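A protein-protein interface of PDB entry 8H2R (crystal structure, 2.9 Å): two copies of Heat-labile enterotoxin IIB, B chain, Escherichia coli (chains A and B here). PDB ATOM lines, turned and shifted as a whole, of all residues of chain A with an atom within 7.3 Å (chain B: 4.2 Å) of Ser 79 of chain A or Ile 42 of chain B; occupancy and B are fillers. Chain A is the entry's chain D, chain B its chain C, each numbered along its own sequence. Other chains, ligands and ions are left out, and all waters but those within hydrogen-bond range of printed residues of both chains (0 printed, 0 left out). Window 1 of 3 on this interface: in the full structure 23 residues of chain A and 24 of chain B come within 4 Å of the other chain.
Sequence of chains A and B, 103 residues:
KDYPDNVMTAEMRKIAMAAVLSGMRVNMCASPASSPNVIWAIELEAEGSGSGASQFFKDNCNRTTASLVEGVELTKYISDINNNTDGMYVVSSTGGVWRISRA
Printed residues of chain B within 4 Å of Asp 80 of chain A: Met 8 and Ala 41.
Of the printed residues of chain B, Ile 81 of chain A touches Met 8 (3.4 Å).
Of the printed residues of chain B, Gly 87 of chain A touches Met 8 (3.8 Å).
Of the printed residues of chain A, Met 12 of chain B touches Ser 79.
Asn 27 of chain B touches none of the printed residues of chain A.
Printed residues of chain A within 4 Å of Ile 42 of chain B: Tyr 77, Ile 78 and Ser 79.
The nearest printed residue of chain B that does not touch Ser 79 of chain A is Glu 43 of chain B (5.1 Å).
The nearest printed residue of chain A that does not touch Ile 42 of chain B is Asp 80 of chain A (5.2 Å).
ND2 of Asn 27 of chain B is in hydrogen-bond range of OE2 of Glu 43 of chain B.
The backbone NH of Ile 78 of chain A is in hydrogen-bond range of the backbone carbonyl oxygen of Tyr 89 of chain A (2.7 Å).
The backbone NH of Asn 82 of chain A is in hydrogen-bond range of the side-chain carboxylate of Asp 80 of chain A (2.6 Å).
The side-chain carboxylate (OD1) of Asp 80 of chain A sits close to the backbone carbonyl oxygen (O) of Thr 85 of chain A (2.7 Å).
The backbone carbonyl oxygen (O) of Asp 80 of chain A sits at hydrogen-bond distance from the backbone NH (N) of Gly 87 of chain A, 3.0 Å away.
The backbone carbonyl oxygen (O) of Met 8 of chain B is in hydrogen-bond range of the side-chain hydroxyl (OG) of Ser 79 of chain A (3.0 Å).
O of Ile 42 of chain B sits at hydrogen-bond distance from N of Ser 79 of chain A (2.9 Å).
Hydrophobic or aromatic side chains of chain B that line the printed part of chain A: Met 8, Met 12, Ile 15, Ala 41 and Phe 57.
Hydrophobic or aromatic side chains of chain A within 4 Å of the printed part of chain B: Ile 78, Ile 81 and Met 88.
Among the printed residues, no Asp or Glu carboxylate lies within 4 Å of a Lys or Arg side-chain nitrogen of the other chain.
No position is printed for both chains.
Among the printed residues, pairs that only touch across the chains: Tyr 77 of chain A with Ile 15 of chain B (3.7 Å), Tyr 77 of chain A with Ile 42 of chain B (3.99 Å), Tyr 77 of chain A with Glu 43 of chain B (3.1 Å), Ile 78 of chain A with Ile 42 of chain B (3.4 Å), Ile 78 of chain A with Glu 43 of chain B (3.4 Å), Ile 78 of chain A with Phe 57 of chain B (3.8 Å), Ser 79 of chain A with Met 12 of chain B (3.1 Å), Ser 79 of chain A with Ile 15 of chain B (3.8 Å), Ser 79 of chain A with Ala 41 of chain B (3.4 Å), Asp 80 of chain A with Met 8 of chain B (3.3 Å), Asp 80 of chain A with Ala 41 of chain B (3.3 Å), Ile 81 of chain A with Met 8 of chain B (3.4 Å), Asp 86 of chain A with Met 8 of chain B (3.8 Å), Gly 87 of chain A with Met 8 of chain B (3.8 Å) and Met 88 of chain A with Met 8 of chain B (3.4 Å).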
ATOM      1  N   TYR A  77     -19.135  17.079  -3.823  1.00  0.00           N
ATOM      2  CA  TYR A  77     -19.721  17.946  -4.835  1.00  0.00           C
ATOM      3  C   TYR A  77     -19.667  17.211  -6.167  1.00  0.00           C
ATOM      4  O   TYR A  77     -18.594  16.742  -6.562  1.00  0.00           O
ATOM      5  CB  TYR A  77     -18.951  19.277  -4.902  1.00  0.00           C
ATOM      6  CG  TYR A  77     -19.637  20.391  -5.666  1.00  0.00           C
ATOM      7  CD1 TYR A  77     -20.795  20.156  -6.399  1.00  0.00           C
ATOM      8  CD2 TYR A  77     -19.136  21.686  -5.645  1.00  0.00           C
ATOM      9  CE1 TYR A  77     -21.421  21.173  -7.098  1.00  0.00           C
ATOM     10  CE2 TYR A  77     -19.756  22.709  -6.343  1.00  0.00           C
ATOM     11  CZ  TYR A  77     -20.899  22.443  -7.069  1.00  0.00           C
ATOM     12  OH  TYR A  77     -21.537  23.444  -7.770  1.00  0.00           O
ATOM     13  N   ILE A  78     -20.813  17.091  -6.847  1.00  0.00           N
ATOM     14  CA  ILE A  78     -20.909  16.331  -8.098  1.00  0.00           C
ATOM     15  C   ILE A  78     -21.402  17.231  -9.228  1.00  0.00           C
ATOM     16  O   ILE A  78     -22.422  17.915  -9.077  1.00  0.00           O
ATOM     17  CB  ILE A  78     -21.850  15.113  -7.972  1.00  0.00           C
ATOM     18  CG1 ILE A  78     -21.275  14.030  -7.063  1.00  0.00           C
ATOM     19  CG2 ILE A  78     -22.139  14.530  -9.339  1.00  0.00           C
ATOM     20  CD1 ILE A  78     -22.335  13.186  -6.375  1.00  0.00           C
ATOM     21  N   SER A  79     -20.704  17.192 -10.369  1.00  0.00           N
ATOM     22  CA  SER A  79     -21.238  17.684 -11.640  1.00  0.00           C
ATOM     23  C   SER A  79     -21.370  16.536 -12.637  1.00  0.00           C
ATOM     24  O   SER A  79     -20.424  15.770 -12.846  1.00  0.00           O
ATOM     25  CB  SER A  79     -20.365  18.780 -12.249  1.00  0.00           C
ATOM     26  OG  SER A  79     -20.720  18.968 -13.616  1.00  0.00           O
ATOM     27  N   ASP A  80     -22.524  16.442 -13.285  1.00  0.00           N
ATOM     28  CA  ASP A  80     -22.845  15.276 -14.093  1.00  0.00           C
ATOM     29  C   ASP A  80     -23.576  15.713 -15.352  1.00  0.00           C
ATOM     30  O   ASP A  80     -24.491  16.537 -15.288  1.00  0.00           O
ATOM     31  CB  ASP A  80     -23.695  14.282 -13.280  1.00  0.00           C
ATOM     32  CG  ASP A  80     -23.769  12.891 -13.919  1.00  0.00           C
ATOM     33  OD1 ASP A  80     -24.017  12.789 -15.141  1.00  0.00           O
ATOM     34  OD2 ASP A  80     -23.561  11.895 -13.194  1.00  0.00           O
ATOM     35  N   ILE A  81     -23.166  15.166 -16.494  1.00  0.00           N
ATOM     36  CA  ILE A  81     -23.818  15.462 -17.762  1.00  0.00           C
ATOM     37  C   ILE A  81     -24.175  14.166 -18.475  1.00  0.00           C
ATOM     38  O   ILE A  81     -24.188  14.109 -19.709  1.00  0.00           O
ATOM     39  CB  ILE A  81     -22.939  16.346 -18.660  1.00  0.00           C
ATOM     40  CG1 ILE A  81     -21.532  15.767 -18.811  1.00  0.00           C
ATOM     41  CG2 ILE A  81     -22.857  17.719 -18.097  1.00  0.00           C
ATOM     42  CD1 ILE A  81     -21.302  15.020 -20.106  1.00  0.00           C
ATOM     43  N   ASN A  82     -24.471  13.117 -17.714  1.00  0.00           N
ATOM     44  CA  ASN A  82     -25.021  11.908 -18.304  1.00  0.00           C
ATOM     45  C   ASN A  82     -26.494  12.118 -18.607  1.00  0.00           C
ATOM     46  O   ASN A  82     -27.208  12.750 -17.826  1.00  0.00           O
ATOM     47  CB  ASN A  82     -24.836  10.721 -17.367  1.00  0.00           C
ATOM     48  CG  ASN A  82     -23.600   9.924 -17.698  1.00  0.00           C
ATOM     49  OD1 ASN A  82     -23.196   9.846 -18.863  1.00  0.00           O
ATOM     50  ND2 ASN A  82     -22.980   9.333 -16.677  1.00  0.00           N
ATOM     51  N   THR A  85     -28.817  11.624 -16.045  1.00  0.00           N
ATOM     52  CA  THR A  85     -28.360  12.185 -14.780  1.00  0.00           C
ATOM     53  C   THR A  85     -27.615  13.498 -15.031  1.00  0.00           C
ATOM     54  O   THR A  85     -26.490  13.714 -14.581  1.00  0.00           O
ATOM     55  CB  THR A  85     -27.509  11.162 -14.045  1.00  0.00           C
ATOM     56  OG1 THR A  85     -26.683  10.475 -14.990  1.00  0.00           O
ATOM     57  CG2 THR A  85     -28.420  10.146 -13.405  1.00  0.00           C
ATOM     58  N   ASP A  86     -28.247  14.389 -15.781  1.00  0.00           N
ATOM     59  CA  ASP A  86     -27.747  15.743 -15.911  1.00  0.00           C
ATOM     60  C   ASP A  86     -28.162  16.536 -14.685  1.00  0.00           C
ATOM     61  O   ASP A  86     -29.347  16.576 -14.331  1.00  0.00           O
ATOM     62  CB  ASP A  86     -28.287  16.398 -17.181  1.00  0.00           C
ATOM     63  CG  ASP A  86     -27.982  15.589 -18.417  1.00  0.00           C
ATOM     64  OD1 ASP A  86     -26.800  15.534 -18.810  1.00  0.00           O
ATOM     65  OD2 ASP A  86     -28.912  15.002 -19.001  1.00  0.00           O
ATOM     66  N   GLY A  87     -27.191  17.139 -14.023  1.00  0.00           N
ATOM     67  CA  GLY A  87     -27.504  18.016 -12.917  1.00  0.00           C
ATOM     68  C   GLY A  87     -26.322  18.175 -11.991  1.00  0.00           C
ATOM     69  O   GLY A  87     -25.247  17.617 -12.207  1.00  0.00           O
ATOM     70  N   MET A  88     -26.556  18.963 -10.943  1.00  0.00           N
ATOM     71  CA  MET A  88     -25.573  19.227  -9.905  1.00  0.00           C
ATOM     72  C   MET A  88     -26.039  18.570  -8.624  1.00  0.00           C
ATOM     73  O   MET A  88     -27.234  18.573  -8.329  1.00  0.00           O
ATOM     74  CB  MET A  88     -25.398  20.726  -9.666  1.00  0.00           C
ATOM     75  CG  MET A  88     -25.297  21.599 -10.915  1.00  0.00           C
ATOM     76  SD  MET A  88     -23.984  20.983 -11.940  1.00  0.00           S
ATOM     77  CE  MET A  88     -22.667  21.490 -10.873  1.00  0.00           C
ATOM     78  N   TYR A  89     -25.100  18.012  -7.863  1.00  0.00           N
ATOM     79  CA  TYR A  89     -25.455  17.253  -6.670  1.00  0.00           C
ATOM     80  C   TYR A  89     -24.443  17.503  -5.566  1.00  0.00           C
ATOM     81  O   TYR A  89     -23.259  17.759  -5.826  1.00  0.00           O
ATOM     82  CB  TYR A  89     -25.566  15.728  -6.957  1.00  0.00           C
ATOM     83  CG  TYR A  89     -26.568  15.409  -8.051  1.00  0.00           C
ATOM     84  CD1 TYR A  89     -27.920  15.250  -7.756  1.00  0.00           C
ATOM     85  CD2 TYR A  89     -26.172  15.318  -9.388  1.00  0.00           C
ATOM     86  CE1 TYR A  89     -28.844  14.990  -8.759  1.00  0.00           C
ATOM     87  CE2 TYR A  89     -27.092  15.064 -10.396  1.00  0.00           C
ATOM     88  CZ  TYR A  89     -28.424  14.900 -10.070  1.00  0.00           C
ATOM     89  OH  TYR A  89     -29.341  14.650 -11.053  1.00  0.00           O
ATOM     90  N   MET B   8     -22.954  22.897 -16.179  1.00  0.00           N
ATOM     91  CA  MET B   8     -22.347  21.690 -15.634  1.00  0.00           C
ATOM     92  C   MET B   8     -20.861  21.620 -15.964  1.00  0.00           C
ATOM     93  O   MET B   8     -20.019  21.544 -15.060  1.00  0.00           O
ATOM     94  CB  MET B   8     -23.066  20.453 -16.153  1.00  0.00           C
ATOM     95  CG  MET B   8     -24.072  19.850 -15.193  1.00  0.00           C
ATOM     96  SD  MET B   8     -25.759  20.387 -15.494  1.00  0.00           S
ATOM     97  CE  MET B   8     -26.114  19.505 -17.015  1.00  0.00           C
ATOM     98  N   MET B  12     -17.605  21.392 -13.781  1.00  0.00           N
ATOM     99  CA  MET B  12     -16.550  20.395 -13.891  1.00  0.00           C
ATOM    100  C   MET B  12     -15.179  21.060 -13.872  1.00  0.00           C
ATOM    101  O   MET B  12     -14.258  20.574 -13.204  1.00  0.00           O
ATOM    102  CB  MET B  12     -16.736  19.577 -15.163  1.00  0.00           C
ATOM    103  CG  MET B  12     -18.028  18.781 -15.187  1.00  0.00           C
ATOM    104  SD  MET B  12     -18.120  17.472 -16.445  1.00  0.00           S
ATOM    105  CE  MET B  12     -18.877  16.179 -15.477  1.00  0.00           C
ATOM    106  N   ILE B  15     -14.474  22.025 -10.091  1.00  0.00           N
ATOM    107  CA  ILE B  15     -14.107  20.845  -9.310  1.00  0.00           C
ATOM    108  C   ILE B  15     -12.697  20.406  -9.669  1.00  0.00           C
ATOM    109  O   ILE B  15     -11.883  20.084  -8.791  1.00  0.00           O
ATOM    110  CB  ILE B  15     -15.106  19.694  -9.551  1.00  0.00           C
ATOM    111  CG1 ILE B  15     -16.334  19.818  -8.656  1.00  0.00           C
ATOM    112  CG2 ILE B  15     -14.451  18.351  -9.253  1.00  0.00           C
ATOM    113  CD1 ILE B  15     -17.577  19.118  -9.222  1.00  0.00           C
ATOM    114  N   VAL B  26     -10.882  13.185  -6.577  1.00  0.00           N
ATOM    115  CA  VAL B  26     -12.168  13.111  -7.245  1.00  0.00           C
ATOM    116  C   VAL B  26     -12.371  11.686  -7.726  1.00  0.00           C
ATOM    117  O   VAL B  26     -11.424  10.924  -7.922  1.00  0.00           O
ATOM    118  CB  VAL B  26     -12.315  14.104  -8.423  1.00  0.00           C
ATOM    119  CG1 VAL B  26     -11.853  15.471  -8.029  1.00  0.00           C
ATOM    120  CG2 VAL B  26     -11.586  13.611  -9.640  1.00  0.00           C
ATOM    121  N   ASN B  27     -13.633  11.321  -7.860  1.00  0.00           N
ATOM    122  CA  ASN B  27     -14.052  10.134  -8.572  1.00  0.00           C
ATOM    123  C   ASN B  27     -14.683  10.587  -9.880  1.00  0.00           C
ATOM    124  O   ASN B  27     -15.203  11.695  -9.984  1.00  0.00           O
ATOM    125  CB  ASN B  27     -15.035   9.299  -7.745  1.00  0.00           C
ATOM    126  CG  ASN B  27     -14.666   9.250  -6.263  1.00  0.00           C
ATOM    127  OD1 ASN B  27     -13.687   8.611  -5.858  1.00  0.00           O
ATOM    128  ND2 ASN B  27     -15.465   9.921  -5.442  1.00  0.00           N
ATOM    129  N   MET B  28     -14.612   9.742 -10.896  1.00  0.00           N
ATOM    130  CA  MET B  28     -14.925  10.187 -12.243  1.00  0.00           C
ATOM    131  C   MET B  28     -15.654   9.100 -13.004  1.00  0.00           C
ATOM    132  O   MET B  28     -15.237   7.938 -13.003  1.00  0.00           O
ATOM    133  CB  MET B  28     -13.655  10.603 -12.989  1.00  0.00           C
ATOM    134  CG  MET B  28     -12.921  11.807 -12.379  1.00  0.00           C
ATOM    135  SD  MET B  28     -11.579  12.407 -13.425  1.00  0.00           S
ATOM    136  CE  MET B  28     -11.960  11.524 -14.886  1.00  0.00           C
ATOM    137  N   ALA B  41     -18.706  12.627 -15.653  1.00  0.00           N
ATOM    138  CA  ALA B  41     -19.186  13.012 -14.331  1.00  0.00           C
ATOM    139  C   ALA B  41     -17.995  13.021 -13.386  1.00  0.00           C
ATOM    140  O   ALA B  41     -17.190  12.080 -13.370  1.00  0.00           O
ATOM    141  CB  ALA B  41     -20.296  12.083 -13.816  1.00  0.00           C
ATOM    142  N   ILE B  42     -17.875  14.097 -12.623  1.00  0.00           N
ATOM    143  CA  ILE B  42     -16.833  14.243 -11.628  1.00  0.00           C
ATOM    144  C   ILE B  42     -17.490  14.548 -10.296  1.00  0.00           C
ATOM    145  O   ILE B  42     -18.540  15.202 -10.240  1.00  0.00           O
ATOM    146  CB  ILE B  42     -15.824  15.327 -12.049  1.00  0.00           C
ATOM    147  CG1 ILE B  42     -14.470  15.117 -11.394  1.00  0.00           C
ATOM    148  CG2 ILE B  42     -16.359  16.702 -11.795  1.00  0.00           C
ATOM    149  CD1 ILE B  42     -13.453  16.054 -11.921  1.00  0.00           C
ATOM    150  N   GLU B  43     -16.910  14.005  -9.231  1.00  0.00           N
ATOM    151  CA  GLU B  43     -17.368  14.236  -7.866  1.00  0.00           C
ATOM    152  C   GLU B  43     -16.159  14.665  -7.056  1.00  0.00           C
ATOM    153  O   GLU B  43     -15.140  13.970  -7.053  1.00  0.00           O
ATOM    154  CB  GLU B  43     -18.017  12.983  -7.263  1.00  0.00           C
ATOM    155  CG  GLU B  43     -17.687  12.711  -5.793  1.00  0.00           C
ATOM    156  CD  GLU B  43     -18.338  11.414  -5.251  1.00  0.00           C
ATOM    157  OE1 GLU B  43     -19.536  11.179  -5.555  1.00  0.00           O
ATOM    158  OE2 GLU B  43     -17.661  10.645  -4.504  1.00  0.00           O
ATOM    159  N   PHE B  57     -23.270   8.547  -6.628  1.00  0.00           N
ATOM    160  CA  PHE B  57     -22.387   8.631  -7.789  1.00  0.00           C
ATOM    161  C   PHE B  57     -22.233   7.288  -8.479  1.00  0.00           C
ATOM    162  O   PHE B  57     -22.209   7.223  -9.712  1.00  0.00           O
ATOM    163  CB  PHE B  57     -21.005   9.166  -7.419  1.00  0.00           C
ATOM    164  CG  PHE B  57     -20.195   9.608  -8.623  1.00  0.00           C
ATOM    165  CD1 PHE B  57     -19.642   8.685  -9.505  1.00  0.00           C
ATOM    166  CD2 PHE B  57     -20.026  10.954  -8.903  1.00  0.00           C
ATOM    167  CE1 PHE B  57     -18.920   9.106 -10.625  1.00  0.00           C
ATOM    168  CE2 PHE B  57     -19.297  11.376 -10.023  1.00  0.00           C
ATOM    169  CZ  PHE B  57     -18.746  10.450 -10.874  1.00  0.00           C
